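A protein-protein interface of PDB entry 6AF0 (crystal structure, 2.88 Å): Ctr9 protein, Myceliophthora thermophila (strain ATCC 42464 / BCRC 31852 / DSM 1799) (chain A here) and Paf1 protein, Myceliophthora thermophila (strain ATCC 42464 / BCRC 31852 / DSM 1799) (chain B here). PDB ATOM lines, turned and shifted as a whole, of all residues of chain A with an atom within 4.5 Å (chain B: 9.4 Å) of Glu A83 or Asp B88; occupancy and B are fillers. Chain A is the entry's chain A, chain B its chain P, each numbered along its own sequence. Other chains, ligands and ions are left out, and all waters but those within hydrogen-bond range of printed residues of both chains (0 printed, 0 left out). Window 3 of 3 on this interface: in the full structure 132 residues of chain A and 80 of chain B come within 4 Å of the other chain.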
ATOM      1  N   ARG A  47      -9.943  -1.347  -8.559  1.00  0.00           N
ATOM      2  CA  ARG A  47     -11.040  -0.840  -9.378  1.00  0.00           C
ATOM      3  C   ARG A  47     -11.353  -1.701 -10.591  1.00  0.00           C
ATOM      4  O   ARG A  47     -12.466  -1.679 -11.093  1.00  0.00           O
ATOM      5  CB  ARG A  47     -10.724   0.577  -9.826  1.00  0.00           C
ATOM      6  CG  ARG A  47      -9.669   1.259  -8.957  1.00  0.00           C
ATOM      7  CD  ARG A  47      -9.395   2.687  -9.390  1.00  0.00           C
ATOM      8  NE  ARG A  47      -8.170   3.231  -8.801  1.00  0.00           N
ATOM      9  CZ  ARG A  47      -6.956   3.168  -9.355  1.00  0.00           C
ATOM     10  NH1 ARG A  47      -6.755   2.590 -10.538  1.00  0.00           N
ATOM     11  NH2 ARG A  47      -5.921   3.685  -8.712  1.00  0.00           N
ATOM     12  N   MET A  51     -15.302  -2.895 -11.876  1.00  0.00           N
ATOM     13  CA  MET A  51     -15.718  -2.782 -13.267  1.00  0.00           C
ATOM     14  C   MET A  51     -15.995  -4.153 -13.879  1.00  0.00           C
ATOM     15  O   MET A  51     -17.038  -4.351 -14.500  1.00  0.00           O
ATOM     16  CB  MET A  51     -14.660  -2.050 -14.086  1.00  0.00           C
ATOM     17  CG  MET A  51     -14.648  -0.550 -13.843  1.00  0.00           C
ATOM     18  SD  MET A  51     -15.572   0.421 -15.055  1.00  0.00           S
ATOM     19  CE  MET A  51     -14.379   0.391 -16.401  1.00  0.00           C
ATOM     20  N   GLN A  81      -9.111  10.011  -8.956  1.00  0.00           N
ATOM     21  CA  GLN A  81     -10.085  10.367 -10.000  1.00  0.00           C
ATOM     22  C   GLN A  81      -9.748   9.807 -11.395  1.00  0.00           C
ATOM     23  O   GLN A  81     -10.431  10.131 -12.366  1.00  0.00           O
ATOM     24  CB  GLN A  81     -10.206  11.894 -10.131  1.00  0.00           C
ATOM     25  CG  GLN A  81     -10.392  12.674  -8.837  1.00  0.00           C
ATOM     26  CD  GLN A  81      -9.075  13.044  -8.173  1.00  0.00           C
ATOM     27  OE1 GLN A  81      -8.008  12.969  -8.789  1.00  0.00           O
ATOM     28  NE2 GLN A  81      -9.144  13.460  -6.909  1.00  0.00           N
ATOM     29  N   ARG A  82      -8.710   8.980 -11.502  1.00  0.00           N
ATOM     30  CA  ARG A  82      -8.250   8.486 -12.807  1.00  0.00           C
ATOM     31  C   ARG A  82      -9.089   7.325 -13.325  1.00  0.00           C
ATOM     32  O   ARG A  82      -9.456   7.292 -14.504  1.00  0.00           O
ATOM     33  CB  ARG A  82      -6.763   8.111 -12.758  1.00  0.00           C
ATOM     34  CG  ARG A  82      -5.844   9.235 -12.273  1.00  0.00           C
ATOM     35  CD  ARG A  82      -6.451  10.618 -12.507  1.00  0.00           C
ATOM     36  NE  ARG A  82      -5.503  11.726 -12.415  1.00  0.00           N
ATOM     37  CZ  ARG A  82      -5.789  12.992 -12.737  1.00  0.00           C
ATOM     38  NH1 ARG A  82      -6.999  13.336 -13.191  1.00  0.00           N
ATOM     39  NH2 ARG A  82      -4.855  13.926 -12.614  1.00  0.00           N
ATOM     40  N   GLU A  83      -9.397   6.380 -12.446  1.00  0.00           N
ATOM     41  CA  GLU A  83     -10.406   5.369 -12.765  1.00  0.00           C
ATOM     42  C   GLU A  83     -11.761   5.785 -12.224  1.00  0.00           C
ATOM     43  O   GLU A  83     -12.774   5.262 -12.679  1.00  0.00           O
ATOM     44  CB  GLU A  83     -10.020   4.000 -12.208  1.00  0.00           C
ATOM     45  CG  GLU A  83     -10.897   2.808 -12.630  1.00  0.00           C
ATOM     46  CD  GLU A  83     -10.771   2.446 -14.100  1.00  0.00           C
ATOM     47  OE1 GLU A  83      -9.696   2.665 -14.685  1.00  0.00           O
ATOM     48  OE2 GLU A  83     -11.744   1.936 -14.690  1.00  0.00           O
ATOM     49  N   LYS A  84     -11.799   6.714 -11.269  1.00  0.00           N
ATOM     50  CA  LYS A  84     -13.082   7.300 -10.880  1.00  0.00           C
ATOM     51  C   LYS A  84     -13.758   7.837 -12.156  1.00  0.00           C
ATOM     52  O   LYS A  84     -14.940   7.571 -12.421  1.00  0.00           O
ATOM     53  CB  LYS A  84     -12.911   8.420  -9.858  1.00  0.00           C
ATOM     54  CG  LYS A  84     -13.947   8.426  -8.741  1.00  0.00           C
ATOM     55  CD  LYS A  84     -14.370   9.829  -8.320  1.00  0.00           C
ATOM     56  CE  LYS A  84     -15.414   9.759  -7.210  1.00  0.00           C
ATOM     57  NZ  LYS A  84     -15.940  11.102  -6.852  1.00  0.00           N
ATOM     58  N   LEU A  85     -12.976   8.567 -12.954  1.00  0.00           N
ATOM     59  CA  LEU A  85     -13.409   9.043 -14.269  1.00  0.00           C
ATOM     60  C   LEU A  85     -14.030   7.923 -15.084  1.00  0.00           C
ATOM     61  O   LEU A  85     -15.113   8.067 -15.627  1.00  0.00           O
ATOM     62  CB  LEU A  85     -12.220   9.623 -15.034  1.00  0.00           C
ATOM     63  CG  LEU A  85     -12.438   9.821 -16.535  1.00  0.00           C
ATOM     64  CD1 LEU A  85     -13.421  10.952 -16.798  1.00  0.00           C
ATOM     65  CD2 LEU A  85     -11.115  10.094 -17.220  1.00  0.00           C
ATOM     66  N   GLY A  86     -13.312   6.813 -15.176  1.00  0.00           N
ATOM     67  CA  GLY A  86     -13.830   5.613 -15.838  1.00  0.00           C
ATOM     68  C   GLY A  86     -15.213   5.199 -15.352  1.00  0.00           C
ATOM     69  O   GLY A  86     -16.194   5.323 -16.062  1.00  0.00           O
ATOM     70  N   ILE A  87     -15.296   4.710 -14.128  1.00  0.00           N
ATOM     71  CA  ILE A  87     -16.571   4.235 -13.590  1.00  0.00           C
ATOM     72  C   ILE A  87     -17.696   5.288 -13.669  1.00  0.00           C
ATOM     73  O   ILE A  87     -18.830   4.953 -13.965  1.00  0.00           O
ATOM     74  CB  ILE A  87     -16.426   3.627 -12.166  1.00  0.00           C
ATOM     75  CG1 ILE A  87     -15.635   4.536 -11.220  1.00  0.00           C
ATOM     76  CG2 ILE A  87     -15.746   2.265 -12.230  1.00  0.00           C
ATOM     77  CD1 ILE A  87     -16.476   5.578 -10.510  1.00  0.00           C
ATOM     78  N   PHE A 139     -12.845  13.778 -22.521  1.00  0.00           N
ATOM     79  CA  PHE A 139     -12.556  12.372 -22.603  1.00  0.00           C
ATOM     80  C   PHE A 139     -13.530  11.884 -23.667  1.00  0.00           C
ATOM     81  O   PHE A 139     -14.722  11.982 -23.484  1.00  0.00           O
ATOM     82  CB  PHE A 139     -12.892  11.779 -21.252  1.00  0.00           C
ATOM     83  CG  PHE A 139     -12.568  10.345 -21.116  1.00  0.00           C
ATOM     84  CD1 PHE A 139     -11.420   9.841 -21.633  1.00  0.00           C
ATOM     85  CD2 PHE A 139     -13.416   9.511 -20.451  1.00  0.00           C
ATOM     86  CE1 PHE A 139     -11.122   8.516 -21.501  1.00  0.00           C
ATOM     87  CE2 PHE A 139     -13.131   8.184 -20.314  1.00  0.00           C
ATOM     88  CZ  PHE A 139     -11.979   7.686 -20.841  1.00  0.00           C
ATOM     89  N   LEU B  80     -21.746   2.315 -25.348  1.00  0.00           N
ATOM     90  CA  LEU B  80     -20.384   1.810 -25.271  1.00  0.00           C
ATOM     91  C   LEU B  80     -20.283   0.658 -24.293  1.00  0.00           C
ATOM     92  O   LEU B  80     -19.289  -0.071 -24.277  1.00  0.00           O
ATOM     93  CB  LEU B  80     -19.467   2.898 -24.802  1.00  0.00           C
ATOM     94  CG  LEU B  80     -19.702   4.228 -25.480  1.00  0.00           C
ATOM     95  CD1 LEU B  80     -19.908   5.217 -24.387  1.00  0.00           C
ATOM     96  CD2 LEU B  80     -18.526   4.639 -26.317  1.00  0.00           C
ATOM     97  N   MET B  83     -18.232  -2.614 -24.456  1.00  0.00           N
ATOM     98  CA  MET B  83     -17.317  -2.468 -25.574  1.00  0.00           C
ATOM     99  C   MET B  83     -15.901  -2.489 -25.024  1.00  0.00           C
ATOM    100  O   MET B  83     -15.547  -1.600 -24.246  1.00  0.00           O
ATOM    101  CB  MET B  83     -17.612  -1.154 -26.290  1.00  0.00           C
ATOM    102  CG  MET B  83     -17.881  -1.310 -27.776  1.00  0.00           C
ATOM    103  SD  MET B  83     -19.273  -2.370 -28.176  1.00  0.00           S
ATOM    104  CE  MET B  83     -19.519  -1.972 -29.907  1.00  0.00           C
ATOM    105  N   PRO B  84     -15.077  -3.480 -25.424  1.00  0.00           N
ATOM    106  CA  PRO B  84     -14.033  -3.969 -24.510  1.00  0.00           C
ATOM    107  C   PRO B  84     -13.172  -3.002 -23.702  1.00  0.00           C
ATOM    108  O   PRO B  84     -13.082  -3.186 -22.496  1.00  0.00           O
ATOM    109  CB  PRO B  84     -13.181  -4.847 -25.402  1.00  0.00           C
ATOM    110  CG  PRO B  84     -14.206  -5.455 -26.282  1.00  0.00           C
ATOM    111  CD  PRO B  84     -15.038  -4.250 -26.669  1.00  0.00           C
ATOM    112  N   GLY B  85     -12.551  -1.998 -24.292  1.00  0.00           N
ATOM    113  CA  GLY B  85     -11.625  -1.172 -23.503  1.00  0.00           C
ATOM    114  C   GLY B  85     -12.018   0.271 -23.261  1.00  0.00           C
ATOM    115  O   GLY B  85     -11.286   0.999 -22.607  1.00  0.00           O
ATOM    116  N   VAL B  86     -13.169   0.686 -23.784  1.00  0.00           N
ATOM    117  CA  VAL B  86     -13.461   2.126 -23.978  1.00  0.00           C
ATOM    118  C   VAL B  86     -13.455   3.011 -22.733  1.00  0.00           C
ATOM    119  O   VAL B  86     -13.181   4.209 -22.809  1.00  0.00           O
ATOM    120  CB  VAL B  86     -14.803   2.338 -24.687  1.00  0.00           C
ATOM    121  CG1 VAL B  86     -14.679   1.926 -26.138  1.00  0.00           C
ATOM    122  CG2 VAL B  86     -15.911   1.571 -23.985  1.00  0.00           C
ATOM    123  N   PHE B  87     -13.783   2.428 -21.599  1.00  0.00           N
ATOM    124  CA  PHE B  87     -13.841   3.169 -20.355  1.00  0.00           C
ATOM    125  C   PHE B  87     -12.463   3.397 -19.763  1.00  0.00           C
ATOM    126  O   PHE B  87     -12.247   4.334 -18.994  1.00  0.00           O
ATOM    127  CB  PHE B  87     -14.718   2.410 -19.391  1.00  0.00           C
ATOM    128  CG  PHE B  87     -16.152   2.407 -19.791  1.00  0.00           C
ATOM    129  CD1 PHE B  87     -16.778   3.603 -20.092  1.00  0.00           C
ATOM    130  CD2 PHE B  87     -16.872   1.215 -19.882  1.00  0.00           C
ATOM    131  CE1 PHE B  87     -18.096   3.627 -20.456  1.00  0.00           C
ATOM    132  CE2 PHE B  87     -18.202   1.230 -20.242  1.00  0.00           C
ATOM    133  CZ  PHE B  87     -18.812   2.441 -20.527  1.00  0.00           C
ATOM    134  N   ASP B  88     -11.551   2.498 -20.126  1.00  0.00           N
ATOM    135  CA  ASP B  88     -10.116   2.718 -20.030  1.00  0.00           C
ATOM    136  C   ASP B  88      -9.775   3.471 -21.310  1.00  0.00           C
ATOM    137  O   ASP B  88     -10.657   4.043 -21.969  1.00  0.00           O
ATOM    138  CB  ASP B  88      -9.369   1.383 -20.004  1.00  0.00           C
ATOM    139  CG  ASP B  88      -9.918   0.427 -18.959  1.00  0.00           C
ATOM    140  OD1 ASP B  88     -10.504   0.900 -17.949  1.00  0.00           O
ATOM    141  OD2 ASP B  88      -9.767  -0.799 -19.149  1.00  0.00           O
ATOM    142  N   GLY B  89      -8.503   3.483 -21.677  1.00  0.00           N
ATOM    143  CA  GLY B  89      -8.075   4.279 -22.826  1.00  0.00           C
ATOM    144  C   GLY B  89      -8.654   4.040 -24.218  1.00  0.00           C
ATOM    145  O   GLY B  89      -8.876   5.000 -24.949  1.00  0.00           O
ATOM    146  N   ASP B  90      -8.896   2.789 -24.608  1.00  0.00           N
ATOM    147  CA  ASP B  90      -8.929   2.496 -26.049  1.00  0.00           C
ATOM    148  C   ASP B  90     -10.332   2.403 -26.657  1.00  0.00           C
ATOM    149  O   ASP B  90     -11.190   1.656 -26.178  1.00  0.00           O
ATOM    150  CB  ASP B  90      -8.027   1.284 -26.401  1.00  0.00           C
ATOM    151  CG  ASP B  90      -8.778  -0.037 -26.453  1.00  0.00           C
ATOM    152  OD1 ASP B  90      -9.688  -0.173 -27.291  1.00  0.00           O
ATOM    153  OD2 ASP B  90      -8.443  -0.959 -25.687  1.00  0.00           O
ATOM    154  N   GLU B  91     -10.539   3.181 -27.722  1.00  0.00           N
ATOM    155  CA  GLU B  91     -11.726   3.072 -28.554  1.00  0.00           C
ATOM    156  C   GLU B  91     -11.494   2.061 -29.686  1.00  0.00           C
ATOM    157  O   GLU B  91     -12.227   2.072 -30.650  1.00  0.00           O
ATOM    158  CB  GLU B  91     -12.141   4.422 -29.180  1.00  0.00           C
ATOM    159  CG  GLU B  91     -12.092   5.674 -28.296  1.00  0.00           C
ATOM    160  CD  GLU B  91     -12.184   6.988 -29.103  1.00  0.00           C
ATOM    161  OE1 GLU B  91     -12.827   7.037 -30.176  1.00  0.00           O
ATOM    162  OE2 GLU B  91     -11.591   8.000 -28.668  1.00  0.00           O
ATOM    163  N   SER B  92     -10.502   1.183 -29.586  1.00  0.00           N
ATOM    164  CA  SER B  92     -10.277   0.195 -30.646  1.00  0.00           C
ATOM    165  C   SER B  92     -11.603  -0.408 -31.145  1.00  0.00           C
ATOM    166  O   SER B  92     -11.871  -0.412 -32.347  1.00  0.00           O
ATOM    167  CB  SER B  92      -9.336  -0.937 -30.189  1.00  0.00           C
ATOM    168  OG  SER B  92      -8.207  -0.421 -29.508  1.00  0.00           O
ATOM    169  N   SER B  93     -12.438  -0.877 -30.216  1.00  0.00           N
ATOM    170  CA  SER B  93     -13.615  -1.687 -30.546  1.00  0.00           C
ATOM    171  C   SER B  93     -14.571  -0.984 -31.485  1.00  0.00           C
ATOM    172  O   SER B  93     -15.195  -1.624 -32.343  1.00  0.00           O
ATOM    173  CB  SER B  93     -14.361  -2.077 -29.267  1.00  0.00           C
ATOM    174  OG  SER B  93     -14.624  -0.947 -28.445  1.00  0.00           O
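Printed residues of chain B within 4 Å of Met A51: Phe B87. Of the printed residues of chain B, Phe A139 touches Phe B87. Of the printed residues of chain A, Phe B87 touches Met A51, Gly A86 and Phe A139. Asp B88 touches just one residue of chain A: Glu A83 (3.6 Å). The nearest residue of chain B that does not touch Glu A83 is Phe B87 (5.0 Å). The nearest residue of chain A that does not touch Asp B88 is Phe A139 (4.04 Å). The nearest printed residue of chain B that does not touch Met A51 is Asp B88 (4.2 Å).
Among the printed residues, pairs that only touch across the chains: Met A51 with Phe B87, Glu A83 with Asp B88, Gly A86 with Phe B87 and Phe A139 with Phe B87.
Of the 12 printed residues of chain B, 2 touch a printed residue of chain A. Of the 10 printed residues of chain A, 4 touch a printed residue of chain B. Hydrophobic or aromatic side chains of chain A that line the printed part of chain B: Met A51 and Phe A139. Among the printed residues, no Asp or Glu carboxylate lies within 4 Å of a Lys or Arg side-chain nitrogen of the other chain.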
